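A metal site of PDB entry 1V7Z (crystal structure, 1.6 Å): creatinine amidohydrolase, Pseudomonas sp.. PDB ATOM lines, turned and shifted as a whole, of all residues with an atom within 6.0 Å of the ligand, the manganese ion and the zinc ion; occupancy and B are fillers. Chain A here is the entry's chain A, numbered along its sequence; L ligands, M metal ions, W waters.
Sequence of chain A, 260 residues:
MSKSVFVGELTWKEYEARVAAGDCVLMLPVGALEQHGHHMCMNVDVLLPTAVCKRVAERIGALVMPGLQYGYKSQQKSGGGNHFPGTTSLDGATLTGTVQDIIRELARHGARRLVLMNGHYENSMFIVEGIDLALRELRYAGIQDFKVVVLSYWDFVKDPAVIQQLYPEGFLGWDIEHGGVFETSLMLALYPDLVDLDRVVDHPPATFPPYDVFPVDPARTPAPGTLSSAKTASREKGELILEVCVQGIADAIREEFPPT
Within 4 Å of the manganese ion: Glu 34, Asp 45 and His 120.
Water W1 lies within hydrogen-bond range of the side-chain carboxylate of Glu 122 (2.7 Å), the side-chain carboxylate of Glu 34 (2.8 Å) and a nitrogen (N3) of the ligand (3.0 Å).
His 178 touches the zinc ion (ND1 to ZN, 3.9 Å).
Four residues have an atom within 4 Å of the zinc ion: His 36, Asp 45, His 178 and Glu 183.
The nearest printed residue that does not touch the zinc ion is Val 44 (4.1 Å).
A nitrogen (N1) of the ligand sits close to the backbone carbonyl oxygen (O) of Glu 177.
Gly 119 touches the ligand.
Trp 154 touches the ligand (CH2 to C3, 3.8 Å).
Hydrophobic or aromatic side chains that line the ligand: Tyr 121, Trp 154 and His 178.
Of the 22 residues printed, 13 come within 4 Å of the ligand.
The nearest printed residue that does not touch the ligand is Glu 122 (4.3 Å).
The manganese ion is bound by OD2 of Asp 45, OE2 of Glu 34, ND1 of His 120, water W1, O2 of the ligand and O1 of the ligand.
The manganese ion has six donor atoms within binding distance.
A nitrogen (N2) of the ligand lies within hydrogen-bond range of the backbone carbonyl oxygen (O) of Trp 174 (2.8 Å).
A ring nitrogen (ND1) of His 178 is in hydrogen-bond range of a nitrogen (N3) of the ligand (3.3 Å).
N of Tyr 121 sits close to O1 of the ligand.
The backbone carbonyl oxygen of Ser 78 lies within hydrogen-bond range of a nitrogen (N3) of the ligand, at 2.6 Å.
A nitrogen (N2) of the ligand sits at hydrogen-bond distance from the backbone carbonyl oxygen of Asp 175 (3.0 Å).
A ring nitrogen (NE2) of His 178 lies within hydrogen-bond range of the backbone carbonyl oxygen (O) of Gly 79 (3.3 Å).
The backbone carbonyl oxygen (O) of Glu 34 lies within hydrogen-bond range of a ring nitrogen (ND1) of His 36.
The side-chain carboxylate (OE2) of Glu 183 is in hydrogen-bond range of the backbone NH (N) of Gly 179, at 2.9 Å.
The backbone NH (N) of Leu 227 is in hydrogen-bond range of the backbone carbonyl oxygen (O) of His 178 (3.2 Å).
The side-chain hydroxyl of Ser 78 sits at hydrogen-bond distance from the side-chain carboxylate of Glu 122 (2.7 Å).
N of Phe 182 sits at hydrogen-bond distance from OE2 of Glu 177, at 3.2 Å.
NE2 of His 120 sits close to OE1 of Glu 122 (3.3 Å).
The zinc ion is bound by O2 of the ligand (1.9 Å).
The zinc ion is bound by the side-chain carboxylate (OD1) of Asp 45.
The zinc ion is bound by the side-chain carboxylate (OE1) of Glu 183, at 2.0 Å.
The zinc ion is bound by NE2 of His 36.
The zinc ion has four donor atoms within binding distance.
Slightly farther from the zinc ion lies OE2 of Glu 183 (2.8 Å).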
ATOM      1  N   ALA A  32     -12.279  17.528   1.256  1.00  0.00           N
ATOM      2  CA  ALA A  32     -11.064  17.493   2.064  1.00  0.00           C
ATOM      3  C   ALA A  32     -10.177  16.368   1.575  1.00  0.00           C
ATOM      4  O   ALA A  32     -10.643  15.455   0.893  1.00  0.00           O
ATOM      5  CB  ALA A  32     -11.398  17.268   3.532  1.00  0.00           C
ATOM      6  N   GLU A  34      -8.075  13.805   3.663  1.00  0.00           N
ATOM      7  CA  GLU A  34      -8.119  13.458   5.075  1.00  0.00           C
ATOM      8  C   GLU A  34      -8.033  11.953   5.246  1.00  0.00           C
ATOM      9  O   GLU A  34      -8.671  11.198   4.515  1.00  0.00           O
ATOM     10  CB  GLU A  34      -9.428  13.948   5.674  1.00  0.00           C
ATOM     11  CG  GLU A  34      -9.571  13.740   7.171  1.00  0.00           C
ATOM     12  CD  GLU A  34     -10.951  14.103   7.681  1.00  0.00           C
ATOM     13  OE1 GLU A  34     -11.072  14.597   8.813  1.00  0.00           O
ATOM     14  OE2 GLU A  34     -11.936  13.902   6.934  1.00  0.00           O
ATOM     15  N   HIS A  36      -8.803   8.337   6.328  1.00  0.00           N
ATOM     16  CA  HIS A  36     -10.060   7.626   6.540  1.00  0.00           C
ATOM     17  C   HIS A  36      -9.799   6.155   6.901  1.00  0.00           C
ATOM     18  O   HIS A  36     -10.374   5.251   6.318  1.00  0.00           O
ATOM     19  CB  HIS A  36     -10.928   7.725   5.293  1.00  0.00           C
ATOM     20  CG  HIS A  36     -11.719   9.001   5.208  1.00  0.00           C
ATOM     21  ND1 HIS A  36     -11.216  10.157   4.653  1.00  0.00           N
ATOM     22  CD2 HIS A  36     -12.976   9.287   5.602  1.00  0.00           C
ATOM     23  CE1 HIS A  36     -12.133  11.108   4.702  1.00  0.00           C
ATOM     24  NE2 HIS A  36     -13.220  10.600   5.277  1.00  0.00           N
ATOM     25  N   VAL A  44     -12.055  10.667  -0.042  1.00  0.00           N
ATOM     26  CA  VAL A  44     -13.473  10.334   0.169  1.00  0.00           C
ATOM     27  C   VAL A  44     -14.380  11.558   0.220  1.00  0.00           C
ATOM     28  O   VAL A  44     -15.433  11.584  -0.408  1.00  0.00           O
ATOM     29  CB  VAL A  44     -13.681   9.513   1.478  1.00  0.00           C
ATOM     30  CG1 VAL A  44     -15.161   9.413   1.849  1.00  0.00           C
ATOM     31  CG2 VAL A  44     -13.096   8.114   1.340  1.00  0.00           C
ATOM     32  N   ASP A  45     -13.968  12.590   0.955  1.00  0.00           N
ATOM     33  CA  ASP A  45     -14.814  13.755   1.185  1.00  0.00           C
ATOM     34  C   ASP A  45     -15.020  14.637  -0.055  1.00  0.00           C
ATOM     35  O   ASP A  45     -15.906  15.496  -0.064  1.00  0.00           O
ATOM     36  CB  ASP A  45     -14.242  14.616   2.316  1.00  0.00           C
ATOM     37  CG  ASP A  45     -14.360  13.954   3.678  1.00  0.00           C
ATOM     38  OD1 ASP A  45     -14.841  12.783   3.775  1.00  0.00           O
ATOM     39  OD2 ASP A  45     -13.992  14.541   4.722  1.00  0.00           O
ATOM     40  N   SER A  78     -14.610  14.696  15.391  1.00  0.00           N
ATOM     41  CA  SER A  78     -15.346  14.477  14.149  1.00  0.00           C
ATOM     42  C   SER A  78     -14.545  13.826  13.011  1.00  0.00           C
ATOM     43  O   SER A  78     -15.131  13.295  12.088  1.00  0.00           O
ATOM     44  CB  SER A  78     -15.977  15.790  13.649  1.00  0.00           C
ATOM     45  OG  SER A  78     -15.035  16.855  13.643  1.00  0.00           O
ATOM     46  N   GLY A  79     -13.224  13.897  13.049  1.00  0.00           N
ATOM     47  CA  GLY A  79     -12.394  13.419  11.953  1.00  0.00           C
ATOM     48  C   GLY A  79     -11.079  12.782  12.368  1.00  0.00           C
ATOM     49  O   GLY A  79     -10.232  12.529  11.518  1.00  0.00           O
ATOM     50  N   GLY A 119     -18.930  17.877   2.074  1.00  0.00           N
ATOM     51  CA  GLY A 119     -18.634  16.481   2.341  1.00  0.00           C
ATOM     52  C   GLY A 119     -17.670  16.229   3.486  1.00  0.00           C
ATOM     53  O   GLY A 119     -17.359  15.084   3.775  1.00  0.00           O
ATOM     54  N   HIS A 120     -17.221  17.297   4.162  1.00  0.00           N
ATOM     55  CA  HIS A 120     -16.285  17.193   5.274  1.00  0.00           C
ATOM     56  C   HIS A 120     -16.844  18.013   6.427  1.00  0.00           C
ATOM     57  O   HIS A 120     -17.038  19.228   6.326  1.00  0.00           O
ATOM     58  CB  HIS A 120     -14.932  17.717   4.820  1.00  0.00           C
ATOM     59  CG  HIS A 120     -13.894  17.843   5.900  1.00  0.00           C
ATOM     60  ND1 HIS A 120     -13.236  16.767   6.455  1.00  0.00           N
ATOM     61  CD2 HIS A 120     -13.340  18.954   6.443  1.00  0.00           C
ATOM     62  CE1 HIS A 120     -12.329  17.216   7.312  1.00  0.00           C
ATOM     63  NE2 HIS A 120     -12.355  18.534   7.308  1.00  0.00           N
ATOM     64  N   TYR A 121     -17.152  17.318   7.520  1.00  0.00           N
ATOM     65  CA  TYR A 121     -17.893  17.857   8.644  1.00  0.00           C
ATOM     66  C   TYR A 121     -17.384  19.224   9.108  1.00  0.00           C
ATOM     67  O   TYR A 121     -18.155  20.157   9.325  1.00  0.00           O
ATOM     68  CB  TYR A 121     -17.814  16.862   9.800  1.00  0.00           C
ATOM     69  CG  TYR A 121     -18.782  17.113  10.909  1.00  0.00           C
ATOM     70  CD1 TYR A 121     -20.022  16.472  10.924  1.00  0.00           C
ATOM     71  CD2 TYR A 121     -18.469  17.964  11.960  1.00  0.00           C
ATOM     72  CE1 TYR A 121     -20.922  16.680  11.946  1.00  0.00           C
ATOM     73  CE2 TYR A 121     -19.364  18.179  12.992  1.00  0.00           C
ATOM     74  CZ  TYR A 121     -20.594  17.540  12.981  1.00  0.00           C
ATOM     75  OH  TYR A 121     -21.482  17.743  14.000  1.00  0.00           O
ATOM     76  N   GLU A 122     -16.064  19.335   9.194  1.00  0.00           N
ATOM     77  CA  GLU A 122     -15.419  20.514   9.760  1.00  0.00           C
ATOM     78  C   GLU A 122     -15.500  21.772   8.892  1.00  0.00           C
ATOM     79  O   GLU A 122     -15.206  22.866   9.361  1.00  0.00           O
ATOM     80  CB  GLU A 122     -13.935  20.188  10.014  1.00  0.00           C
ATOM     81  CG  GLU A 122     -13.655  19.229  11.159  1.00  0.00           C
ATOM     82  CD  GLU A 122     -13.705  17.748  10.792  1.00  0.00           C
ATOM     83  OE1 GLU A 122     -14.230  17.369   9.732  1.00  0.00           O
ATOM     84  OE2 GLU A 122     -13.212  16.942  11.611  1.00  0.00           O
ATOM     85  N   TYR A 153     -24.364  16.486   2.865  1.00  0.00           N
ATOM     86  CA  TYR A 153     -25.256  15.537   2.164  1.00  0.00           C
ATOM     87  C   TYR A 153     -25.852  14.470   3.079  1.00  0.00           C
ATOM     88  O   TYR A 153     -26.999  14.039   2.877  1.00  0.00           O
ATOM     89  CB  TYR A 153     -24.581  14.932   0.914  1.00  0.00           C
ATOM     90  CG  TYR A 153     -23.453  13.989   1.236  1.00  0.00           C
ATOM     91  CD1 TYR A 153     -23.679  12.624   1.339  1.00  0.00           C
ATOM     92  CD2 TYR A 153     -22.167  14.460   1.451  1.00  0.00           C
ATOM     93  CE1 TYR A 153     -22.664  11.759   1.652  1.00  0.00           C
ATOM     94  CE2 TYR A 153     -21.145  13.603   1.776  1.00  0.00           C
ATOM     95  CZ  TYR A 153     -21.383  12.250   1.876  1.00  0.00           C
ATOM     96  OH  TYR A 153     -20.361  11.393   2.200  1.00  0.00           O
ATOM     97  N   TRP A 154     -25.104  14.052   4.105  1.00  0.00           N
ATOM     98  CA  TRP A 154     -25.602  13.067   5.076  1.00  0.00           C
ATOM     99  C   TRP A 154     -26.824  13.508   5.871  1.00  0.00           C
ATOM    100  O   TRP A 154     -27.580  12.665   6.343  1.00  0.00           O
ATOM    101  CB  TRP A 154     -24.493  12.637   6.048  1.00  0.00           C
ATOM    102  CG  TRP A 154     -23.779  13.784   6.731  1.00  0.00           C
ATOM    103  CD1 TRP A 154     -24.206  14.497   7.813  1.00  0.00           C
ATOM    104  CD2 TRP A 154     -22.502  14.328   6.367  1.00  0.00           C
ATOM    105  NE1 TRP A 154     -23.280  15.456   8.136  1.00  0.00           N
ATOM    106  CE2 TRP A 154     -22.225  15.375   7.268  1.00  0.00           C
ATOM    107  CE3 TRP A 154     -21.576  14.037   5.360  1.00  0.00           C
ATOM    108  CZ2 TRP A 154     -21.056  16.131   7.203  1.00  0.00           C
ATOM    109  CZ3 TRP A 154     -20.407  14.793   5.295  1.00  0.00           C
ATOM    110  CH2 TRP A 154     -20.165  15.820   6.212  1.00  0.00           C
ATOM    111  N   TRP A 174     -23.746  12.135  13.402  1.00  0.00           N
ATOM    112  CA  TRP A 174     -22.934  12.304  12.200  1.00  0.00           C
ATOM    113  C   TRP A 174     -21.480  12.707  12.510  1.00  0.00           C
ATOM    114  O   TRP A 174     -20.606  12.477  11.694  1.00  0.00           O
ATOM    115  CB  TRP A 174     -23.583  13.310  11.244  1.00  0.00           C
ATOM    116  CG  TRP A 174     -24.890  12.827  10.661  1.00  0.00           C
ATOM    117  CD1 TRP A 174     -26.101  13.443  10.751  1.00  0.00           C
ATOM    118  CD2 TRP A 174     -25.106  11.631   9.908  1.00  0.00           C
ATOM    119  NE1 TRP A 174     -27.065  12.711  10.093  1.00  0.00           N
ATOM    120  CE2 TRP A 174     -26.483  11.590   9.562  1.00  0.00           C
ATOM    121  CE3 TRP A 174     -24.280  10.580   9.480  1.00  0.00           C
ATOM    122  CZ2 TRP A 174     -27.039  10.539   8.822  1.00  0.00           C
ATOM    123  CZ3 TRP A 174     -24.837   9.551   8.734  1.00  0.00           C
ATOM    124  CH2 TRP A 174     -26.208   9.538   8.423  1.00  0.00           C
ATOM    125  N   ASP A 175     -21.243  13.283  13.688  1.00  0.00           N
ATOM    126  CA  ASP A 175     -19.870  13.603  14.134  1.00  0.00           C
ATOM    127  C   ASP A 175     -18.901  12.402  14.205  1.00  0.00           C
ATOM    128  O   ASP A 175     -17.791  12.468  13.684  1.00  0.00           O
ATOM    129  CB  ASP A 175     -19.873  14.359  15.482  1.00  0.00           C
ATOM    130  CG  ASP A 175     -20.705  13.667  16.550  1.00  0.00           C
ATOM    131  OD1 ASP A 175     -20.118  13.262  17.576  1.00  0.00           O
ATOM    132  OD2 ASP A 175     -21.934  13.483  16.442  1.00  0.00           O
ATOM    133  N   ILE A 176     -19.299  11.292  14.837  1.00  0.00           N
ATOM    134  CA  ILE A 176     -18.404  10.132  14.894  1.00  0.00           C
ATOM    135  C   ILE A 176     -18.510   9.219  13.666  1.00  0.00           C
ATOM    136  O   ILE A 176     -17.902   8.146  13.628  1.00  0.00           O
ATOM    137  CB  ILE A 176     -18.569   9.344  16.221  1.00  0.00           C
ATOM    138  CG1 ILE A 176     -19.993   8.800  16.364  1.00  0.00           C
ATOM    139  CG2 ILE A 176     -18.207  10.224  17.396  1.00  0.00           C
ATOM    140  CD1 ILE A 176     -20.036   7.514  17.172  1.00  0.00           C
ATOM    141  N   GLU A 177     -19.247   9.673  12.656  1.00  0.00           N
ATOM    142  CA  GLU A 177     -19.389   8.956  11.406  1.00  0.00           C
ATOM    143  C   GLU A 177     -18.219   9.274  10.473  1.00  0.00           C
ATOM    144  O   GLU A 177     -18.400   9.725   9.334  1.00  0.00           O
ATOM    145  CB  GLU A 177     -20.723   9.311  10.740  1.00  0.00           C
ATOM    146  CG  GLU A 177     -21.201   8.299   9.730  1.00  0.00           C
ATOM    147  CD  GLU A 177     -20.962   6.872  10.169  1.00  0.00           C
ATOM    148  OE1 GLU A 177     -21.584   6.433  11.161  1.00  0.00           O
ATOM    149  OE2 GLU A 177     -20.125   6.197   9.551  1.00  0.00           O
ATOM    150  N   HIS A 178     -17.015   9.033  10.950  1.00  0.00           N
ATOM    151  CA  HIS A 178     -15.817   9.261  10.153  1.00  0.00           C
ATOM    152  C   HIS A 178     -15.174   7.932   9.794  1.00  0.00           C
ATOM    153  O   HIS A 178     -14.594   7.271  10.649  1.00  0.00           O
ATOM    154  CB  HIS A 178     -14.828  10.142  10.902  1.00  0.00           C
ATOM    155  CG  HIS A 178     -13.596  10.410  10.113  1.00  0.00           C
ATOM    156  ND1 HIS A 178     -13.623  11.058   8.895  1.00  0.00           N
ATOM    157  CD2 HIS A 178     -12.305  10.060  10.316  1.00  0.00           C
ATOM    158  CE1 HIS A 178     -12.411  11.107   8.392  1.00  0.00           C
ATOM    159  NE2 HIS A 178     -11.588  10.502   9.236  1.00  0.00           N
ATOM    160  N   GLY A 179     -15.276   7.558   8.524  1.00  0.00           N
ATOM    161  CA  GLY A 179     -14.715   6.317   8.034  1.00  0.00           C
ATOM    162  C   GLY A 179     -15.485   5.087   8.493  1.00  0.00           C
ATOM    163  O   GLY A 179     -14.966   3.981   8.444  1.00  0.00           O
ATOM    164  N   PHE A 182     -21.339   4.613   7.107  1.00  0.00           N
ATOM    165  CA  PHE A 182     -21.953   5.497   6.120  1.00  0.00           C
ATOM    166  C   PHE A 182     -21.041   5.737   4.914  1.00  0.00           C
ATOM    167  O   PHE A 182     -21.401   5.449   3.776  1.00  0.00           O
ATOM    168  CB  PHE A 182     -22.309   6.835   6.786  1.00  0.00           C
ATOM    169  CG  PHE A 182     -22.987   7.807   5.862  1.00  0.00           C
ATOM    170  CD1 PHE A 182     -22.247   8.759   5.186  1.00  0.00           C
ATOM    171  CD2 PHE A 182     -24.370   7.785   5.681  1.00  0.00           C
ATOM    172  CE1 PHE A 182     -22.858   9.665   4.337  1.00  0.00           C
ATOM    173  CE2 PHE A 182     -24.980   8.699   4.826  1.00  0.00           C
ATOM    174  CZ  PHE A 182     -24.219   9.639   4.156  1.00  0.00           C
ATOM    175  N   GLU A 183     -19.852   6.263   5.177  1.00  0.00           N
ATOM    176  CA  GLU A 183     -18.938   6.597   4.086  1.00  0.00           C
ATOM    177  C   GLU A 183     -18.435   5.345   3.396  1.00  0.00           C
ATOM    178  O   GLU A 183     -18.329   5.318   2.178  1.00  0.00           O
ATOM    179  CB  GLU A 183     -17.741   7.405   4.597  1.00  0.00           C
ATOM    180  CG  GLU A 183     -18.110   8.835   4.961  1.00  0.00           C
ATOM    181  CD  GLU A 183     -16.903   9.656   5.379  1.00  0.00           C
ATOM    182  OE1 GLU A 183     -16.740  10.745   4.816  1.00  0.00           O
ATOM    183  OE2 GLU A 183     -16.148   9.226   6.264  1.00  0.00           O
ATOM    184  N   LEU A 227     -13.588   6.853  13.663  1.00  0.00           N
ATOM    185  CA  LEU A 227     -14.308   7.124  14.910  1.00  0.00           C
ATOM    186  C   LEU A 227     -15.390   6.076  15.162  1.00  0.00           C
ATOM    187  O   LEU A 227     -15.958   6.012  16.239  1.00  0.00           O
ATOM    188  CB  LEU A 227     -14.903   8.537  14.889  1.00  0.00           C
ATOM    189  CG  LEU A 227     -13.857   9.673  14.895  1.00  0.00           C
ATOM    190  CD1 LEU A 227     -14.535  11.028  14.946  1.00  0.00           C
ATOM    191  CD2 LEU A 227     -12.867   9.531  16.052  1.00  0.00           C
HETATM  192  O1  LIG L   1     -16.227  14.604   7.185  1.00  0.00           O
HETATM  193  C1  LIG L   1     -16.207  13.361   7.090  1.00  0.00           C
HETATM  194  O2  LIG L   1     -15.140  12.725   6.868  1.00  0.00           O
HETATM  195  C2  LIG L   1     -17.496  12.581   7.293  1.00  0.00           C
HETATM  196  N1  LIG L   1     -18.165  12.871   8.573  1.00  0.00           N
HETATM  197  C3  LIG L   1     -19.631  12.903   8.520  1.00  0.00           C
HETATM  198  C4  LIG L   1     -17.499  13.072   9.715  1.00  0.00           C
HETATM  199  N2  LIG L   1     -18.120  13.279  10.793  1.00  0.00           N
HETATM  200  N3  LIG L   1     -16.155  13.046   9.750  1.00  0.00           N
HETATM  201 MN    MN M   1     -13.881  14.617   6.774  1.00  0.00          MN
HETATM  202 ZN    ZN M   2     -14.987  11.558   5.319  1.00  0.00          ZN
HETATM  203  O   HOH W   1     -13.839  14.837   9.034  1.00  0.00           O
